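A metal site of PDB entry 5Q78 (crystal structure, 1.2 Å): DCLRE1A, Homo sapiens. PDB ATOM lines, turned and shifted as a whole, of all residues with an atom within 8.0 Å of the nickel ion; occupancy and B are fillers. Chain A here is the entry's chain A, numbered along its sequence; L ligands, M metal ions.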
ATOM      1  N   ASP A  18     -22.065  11.705  16.830  1.00  0.00           N
ATOM      2  CA  ASP A  18     -20.649  11.435  17.267  1.00  0.00           C
ATOM      3  C   ASP A  18     -19.756  12.750  17.294  1.00  0.00           C
ATOM      4  O   ASP A  18     -18.580  12.715  16.867  1.00  0.00           O
ATOM      5  CB  ASP A  18     -20.061  10.270  16.560  1.00  0.00           C
ATOM      6  CG  ASP A  18     -20.890   8.947  16.715  1.00  0.00           C
ATOM      7  OD1 ASP A  18     -21.725   8.914  17.613  1.00  0.00           O
ATOM      8  OD2 ASP A  18     -20.545   8.027  15.929  1.00  0.00           O
ATOM      9  N   THR A  34     -23.550   6.979  18.530  1.00  0.00           N
ATOM     10  CA  THR A  34     -23.841   5.657  17.904  1.00  0.00           C
ATOM     11  C   THR A  34     -23.355   4.484  18.779  1.00  0.00           C
ATOM     12  O   THR A  34     -23.976   3.404  18.773  1.00  0.00           O
ATOM     13  CB  THR A  34     -23.252   5.540  16.482  1.00  0.00           C
ATOM     14  OG1 THR A  34     -21.793   5.649  16.541  1.00  0.00           O
ATOM     15  CG2 THR A  34     -23.823   6.558  15.520  1.00  0.00           C
ATOM     16  N   HIS A  35     -22.236   4.667  19.503  1.00  0.00           N
ATOM     17  CA  HIS A  35     -21.603   3.580  20.281  1.00  0.00           C
ATOM     18  C   HIS A  35     -20.563   4.102  21.211  1.00  0.00           C
ATOM     19  O   HIS A  35     -19.997   5.190  20.944  1.00  0.00           O
ATOM     20  CB  HIS A  35     -21.092   2.428  19.350  1.00  0.00           C
ATOM     21  CG  HIS A  35     -19.908   2.757  18.512  1.00  0.00           C
ATOM     22  ND1 HIS A  35     -19.879   3.614  17.421  1.00  0.00           N
ATOM     23  CD2 HIS A  35     -18.647   2.237  18.560  1.00  0.00           C
ATOM     24  CE1 HIS A  35     -18.663   3.580  16.865  1.00  0.00           C
ATOM     25  NE2 HIS A  35     -17.916   2.735  17.527  1.00  0.00           N
ATOM     26  N   PHE A  36     -20.268   3.270  22.227  1.00  0.00           N
ATOM     27  CA  PHE A  36     -19.231   3.655  23.246  1.00  0.00           C
ATOM     28  C   PHE A  36     -17.799   3.283  22.881  1.00  0.00           C
ATOM     29  O   PHE A  36     -17.216   2.367  23.561  1.00  0.00           O
ATOM     30  CB  PHE A  36     -19.667   3.072  24.605  1.00  0.00           C
ATOM     31  CG  PHE A  36     -18.949   3.665  25.810  1.00  0.00           C
ATOM     32  CD1 PHE A  36     -19.350   4.919  26.271  1.00  0.00           C
ATOM     33  CD2 PHE A  36     -17.953   2.973  26.485  1.00  0.00           C
ATOM     34  CE1 PHE A  36     -18.715   5.511  27.421  1.00  0.00           C
ATOM     35  CE2 PHE A  36     -17.300   3.529  27.613  1.00  0.00           C
ATOM     36  CZ  PHE A  36     -17.704   4.753  28.092  1.00  0.00           C
ATOM     37  N   HIS A  37     -17.233   3.906  21.832  1.00  0.00           N
ATOM     38  CA  HIS A  37     -15.815   3.831  21.502  1.00  0.00           C
ATOM     39  C   HIS A  37     -15.247   5.252  21.585  1.00  0.00           C
ATOM     40  O   HIS A  37     -15.882   6.227  21.179  1.00  0.00           O
ATOM     41  CB  HIS A  37     -15.524   3.234  20.107  1.00  0.00           C
ATOM     42  CG  HIS A  37     -15.569   1.711  20.047  1.00  0.00           C
ATOM     43  ND1 HIS A  37     -15.676   0.984  18.866  1.00  0.00           N
ATOM     44  CD2 HIS A  37     -15.465   0.801  21.029  1.00  0.00           C
ATOM     45  CE1 HIS A  37     -15.638  -0.320  19.129  1.00  0.00           C
ATOM     46  NE2 HIS A  37     -15.523  -0.447  20.439  1.00  0.00           N
ATOM     47  N   SER A  38     -14.014   5.383  22.118  1.00  0.00           N
ATOM     48  CA  SER A  38     -13.423   6.704  22.495  1.00  0.00           C
ATOM     49  C   SER A  38     -13.284   7.642  21.334  1.00  0.00           C
ATOM     50  O   SER A  38     -13.549   8.835  21.605  1.00  0.00           O
ATOM     51  CB  SER A  38     -12.164   6.491  23.352  1.00  0.00           C
ATOM     52  OG  SER A  38     -11.160   5.906  22.560  1.00  0.00           O
ATOM     53  N   ASP A  39     -12.996   7.229  20.126  1.00  0.00           N
ATOM     54  CA  ASP A  39     -12.909   8.214  18.967  1.00  0.00           C
ATOM     55  C   ASP A  39     -14.286   8.867  18.755  1.00  0.00           C
ATOM     56  O   ASP A  39     -14.366  10.009  18.196  1.00  0.00           O
ATOM     57  CB  ASP A  39     -12.430   7.612  17.670  1.00  0.00           C
ATOM     58  CG  ASP A  39     -10.852   7.371  17.594  1.00  0.00           C
ATOM     59  OD1 ASP A  39     -10.171   7.792  18.531  1.00  0.00           O
ATOM     60  OD2 ASP A  39     -10.439   6.777  16.596  1.00  0.00           O
ATOM     61  N   HIS A  40     -15.392   8.173  19.124  1.00  0.00           N
ATOM     62  CA  HIS A  40     -16.764   8.676  18.910  1.00  0.00           C
ATOM     63  C   HIS A  40     -17.316   9.420  20.055  1.00  0.00           C
ATOM     64  O   HIS A  40     -18.044  10.451  19.851  1.00  0.00           O
ATOM     65  CB  HIS A  40     -17.680   7.438  18.517  1.00  0.00           C
ATOM     66  CG  HIS A  40     -17.248   6.808  17.256  1.00  0.00           C
ATOM     67  ND1 HIS A  40     -17.848   7.025  16.034  1.00  0.00           N
ATOM     68  CD2 HIS A  40     -16.206   5.981  16.987  1.00  0.00           C
ATOM     69  CE1 HIS A  40     -17.199   6.389  15.093  1.00  0.00           C
ATOM     70  NE2 HIS A  40     -16.172   5.753  15.653  1.00  0.00           N
ATOM     71  N   HIS A  96     -21.771  -4.265  15.463  1.00  0.00           N
ATOM     72  CA  HIS A  96     -20.403  -3.716  15.796  1.00  0.00           C
ATOM     73  C   HIS A  96     -20.144  -4.221  17.190  1.00  0.00           C
ATOM     74  O   HIS A  96     -19.991  -5.478  17.361  1.00  0.00           O
ATOM     75  CB  HIS A  96     -20.343  -2.203  15.565  1.00  0.00           C
ATOM     76  CG  HIS A  96     -19.021  -1.516  15.767  1.00  0.00           C
ATOM     77  ND1 HIS A  96     -17.889  -1.967  15.172  1.00  0.00           N
ATOM     78  CD2 HIS A  96     -18.664  -0.472  16.553  1.00  0.00           C
ATOM     79  CE1 HIS A  96     -16.867  -1.173  15.542  1.00  0.00           C
ATOM     80  NE2 HIS A  96     -17.302  -0.224  16.348  1.00  0.00           N
ATOM     81  N   CYS A  97     -19.955  -3.379  18.183  1.00  0.00           N
ATOM     82  CA  CYS A  97     -19.790  -3.745  19.635  1.00  0.00           C
ATOM     83  C   CYS A  97     -21.124  -3.698  20.348  1.00  0.00           C
ATOM     84  O   CYS A  97     -22.113  -3.175  19.810  1.00  0.00           O
ATOM     85  CB  CYS A  97     -18.761  -2.788  20.260  1.00  0.00           C
ATOM     86  SG  CYS A  97     -19.282  -1.030  20.317  1.00  0.00           S
ATOM     87  N   ALA A 100     -24.048  -0.744  19.946  1.00  0.00           N
ATOM     88  CA  ALA A 100     -23.788   0.037  18.727  1.00  0.00           C
ATOM     89  C   ALA A 100     -25.018   0.031  17.823  1.00  0.00           C
ATOM     90  O   ALA A 100     -25.637  -1.035  17.587  1.00  0.00           O
ATOM     91  CB  ALA A 100     -22.608  -0.472  18.019  1.00  0.00           C
ATOM     92  N   GLY A 117     -23.159   4.657  11.691  1.00  0.00           N
ATOM     93  CA  GLY A 117     -22.139   4.599  12.742  1.00  0.00           C
ATOM     94  C   GLY A 117     -21.002   3.743  12.294  1.00  0.00           C
ATOM     95  O   GLY A 117     -20.653   3.727  11.121  1.00  0.00           O
ATOM     96  N   ASP A 118     -20.409   3.005  13.200  1.00  0.00           N
ATOM     97  CA  ASP A 118     -19.526   1.858  12.858  1.00  0.00           C
ATOM     98  C   ASP A 118     -20.383   0.577  12.724  1.00  0.00           C
ATOM     99  O   ASP A 118     -21.253   0.337  13.583  1.00  0.00           O
ATOM    100  CB  ASP A 118     -18.393   1.635  13.879  1.00  0.00           C
ATOM    101  CG  ASP A 118     -17.246   2.643  13.870  1.00  0.00           C
ATOM    102  OD1 ASP A 118     -17.129   3.423  12.907  1.00  0.00           O
ATOM    103  OD2 ASP A 118     -16.374   2.550  14.762  1.00  0.00           O
ATOM    104  N   PHE A 119     -20.129  -0.197  11.675  1.00  0.00           N
ATOM    105  CA  PHE A 119     -20.955  -1.409  11.459  1.00  0.00           C
ATOM    106  C   PHE A 119     -20.177  -2.521  10.753  1.00  0.00           C
ATOM    107  O   PHE A 119     -19.210  -2.247  10.053  1.00  0.00           O
ATOM    108  CB  PHE A 119     -22.314  -1.088  10.707  1.00  0.00           C
ATOM    109  CG  PHE A 119     -22.343  -1.022   9.185  1.00  0.00           C
ATOM    110  CD1 PHE A 119     -23.394  -1.524   8.447  1.00  0.00           C
ATOM    111  CD2 PHE A 119     -21.325  -0.406   8.435  1.00  0.00           C
ATOM    112  CE1 PHE A 119     -23.480  -1.408   7.077  1.00  0.00           C
ATOM    113  CE2 PHE A 119     -21.385  -0.319   7.034  1.00  0.00           C
ATOM    114  CZ  PHE A 119     -22.482  -0.823   6.374  1.00  0.00           C
ATOM    115  N   ASP A 141     -19.727   3.888   7.145  1.00  0.00           N
ATOM    116  CA  ASP A 141     -18.443   3.410   7.740  1.00  0.00           C
ATOM    117  C   ASP A 141     -17.662   2.696   6.636  1.00  0.00           C
ATOM    118  O   ASP A 141     -17.879   1.553   6.250  1.00  0.00           O
ATOM    119  CB  ASP A 141     -18.721   2.436   8.901  1.00  0.00           C
ATOM    120  CG  ASP A 141     -17.513   1.669   9.378  1.00  0.00           C
ATOM    121  OD1 ASP A 141     -16.364   2.087   9.018  1.00  0.00           O
ATOM    122  OD2 ASP A 141     -17.694   0.678  10.131  1.00  0.00           O
ATOM    123  N   THR A 143     -14.295   2.074   6.791  1.00  0.00           N
ATOM    124  CA  THR A 143     -13.003   1.658   7.321  1.00  0.00           C
ATOM    125  C   THR A 143     -12.215   0.798   6.407  1.00  0.00           C
ATOM    126  O   THR A 143     -10.999   1.060   6.137  1.00  0.00           O
ATOM    127  CB  THR A 143     -13.206   0.941   8.718  1.00  0.00           C
ATOM    128  OG1 THR A 143     -13.788   1.825   9.684  1.00  0.00           O
ATOM    129  CG2 THR A 143     -11.905   0.426   9.310  1.00  0.00           C
ATOM    130  N   SER A 183     -11.047  -1.872  24.729  1.00  0.00           N
ATOM    131  CA  SER A 183     -12.322  -1.197  24.483  1.00  0.00           C
ATOM    132  C   SER A 183     -13.401  -2.271  24.590  1.00  0.00           C
ATOM    133  O   SER A 183     -13.086  -3.503  24.629  1.00  0.00           O
ATOM    134  CB  SER A 183     -12.401  -0.606  23.044  1.00  0.00           C
ATOM    135  OG  SER A 183     -12.261  -1.632  22.079  1.00  0.00           O
ATOM    136  N   ILE A 184     -14.668  -1.927  24.607  1.00  0.00           N
ATOM    137  CA  ILE A 184     -15.729  -2.906  24.441  1.00  0.00           C
ATOM    138  C   ILE A 184     -15.735  -3.421  23.011  1.00  0.00           C
ATOM    139  O   ILE A 184     -15.122  -2.792  22.075  1.00  0.00           O
ATOM    140  CB  ILE A 184     -17.137  -2.360  24.822  1.00  0.00           C
ATOM    141  CG1 ILE A 184     -17.627  -1.240  23.912  1.00  0.00           C
ATOM    142  CG2 ILE A 184     -17.136  -1.955  26.292  1.00  0.00           C
ATOM    143  CD1 ILE A 184     -19.080  -0.926  24.070  1.00  0.00           C
ATOM    144  N   GLU A 296     -14.978  -6.354  13.725  1.00  0.00           N
ATOM    145  CA  GLU A 296     -16.311  -5.749  13.933  1.00  0.00           C
ATOM    146  C   GLU A 296     -16.667  -4.605  12.920  1.00  0.00           C
ATOM    147  O   GLU A 296     -17.575  -3.808  13.141  1.00  0.00           O
ATOM    148  CB  GLU A 296     -16.567  -5.373  15.360  1.00  0.00           C
ATOM    149  CG  GLU A 296     -16.668  -6.620  16.345  1.00  0.00           C
ATOM    150  CD  GLU A 296     -17.036  -6.348  17.790  1.00  0.00           C
ATOM    151  OE1 GLU A 296     -16.865  -5.210  18.284  1.00  0.00           O
ATOM    152  OE2 GLU A 296     -17.466  -7.370  18.449  1.00  0.00           O
ATOM    153  N   HIS A 297     -15.892  -4.599  11.837  1.00  0.00           N
ATOM    154  CA  HIS A 297     -16.195  -3.751  10.651  1.00  0.00           C
ATOM    155  C   HIS A 297     -16.396  -4.590   9.387  1.00  0.00           C
ATOM    156  O   HIS A 297     -15.810  -5.669   9.239  1.00  0.00           O
ATOM    157  CB  HIS A 297     -15.062  -2.690  10.375  1.00  0.00           C
ATOM    158  CG  HIS A 297     -14.858  -1.669  11.434  1.00  0.00           C
ATOM    159  ND1 HIS A 297     -15.537  -0.482  11.506  1.00  0.00           N
ATOM    160  CD2 HIS A 297     -13.904  -1.623  12.431  1.00  0.00           C
ATOM    161  CE1 HIS A 297     -15.071   0.237  12.530  1.00  0.00           C
ATOM    162  NE2 HIS A 297     -14.130  -0.470  13.112  1.00  0.00           N
HETATM  163  C1  LIG L   1     -12.796   1.878  17.020  1.00  0.00           C
HETATM  164  C2  LIG L   1     -13.210   0.826  15.980  1.00  0.00           C
HETATM  165  C3  LIG L   1     -13.545   3.225  16.893  1.00  0.00           C
HETATM  166  O1  LIG L   1     -12.468   0.192  15.234  1.00  0.00           O
HETATM  167  O2  LIG L   1     -14.388   0.559  15.960  1.00  0.00           O
HETATM  168  O3  LIG L   1     -14.790   3.223  16.922  1.00  0.00           O
HETATM  169  O4  LIG L   1     -12.844   4.318  16.903  1.00  0.00           O
HETATM  170 NI    NI M   1     -16.108   1.669  16.767  1.00  0.00          NI
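The side-chain carboxylate (OD2) of Asp 118 lies close to a ring nitrogen (NE2) of His 40. OG1 of Thr 34 lies within hydrogen-bond range of ND1 of His 35. A ring nitrogen (NE2) of His 37 lies within hydrogen-bond range of the backbone carbonyl oxygen (O) of Ile 184. A ring nitrogen (ND1) of His 96 sits at hydrogen-bond distance from the backbone carbonyl oxygen (O) of Glu 296.
Within 4 Å of the nickel ion: His 35, His 37, His 96 and Asp 118. The nearest printed residue that does not touch the nickel ion is His 40 (4.2 Å).
The nickel ion is bound by O3 of the ligand, 2.0 Å away. O2 of the ligand binds the nickel ion, at 2.2 Å. The nickel ion is bound by the side-chain carboxylate (OD2) of Asp 118, 2.2 Å away. NE2 of His 35 binds the nickel ion (2.2 Å). ND1 of His 37 is bound to the nickel ion (2.2 Å). The nickel ion is bound by NE2 of His 96 (2.3 Å). The nickel ion has six donor atoms within binding distance.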
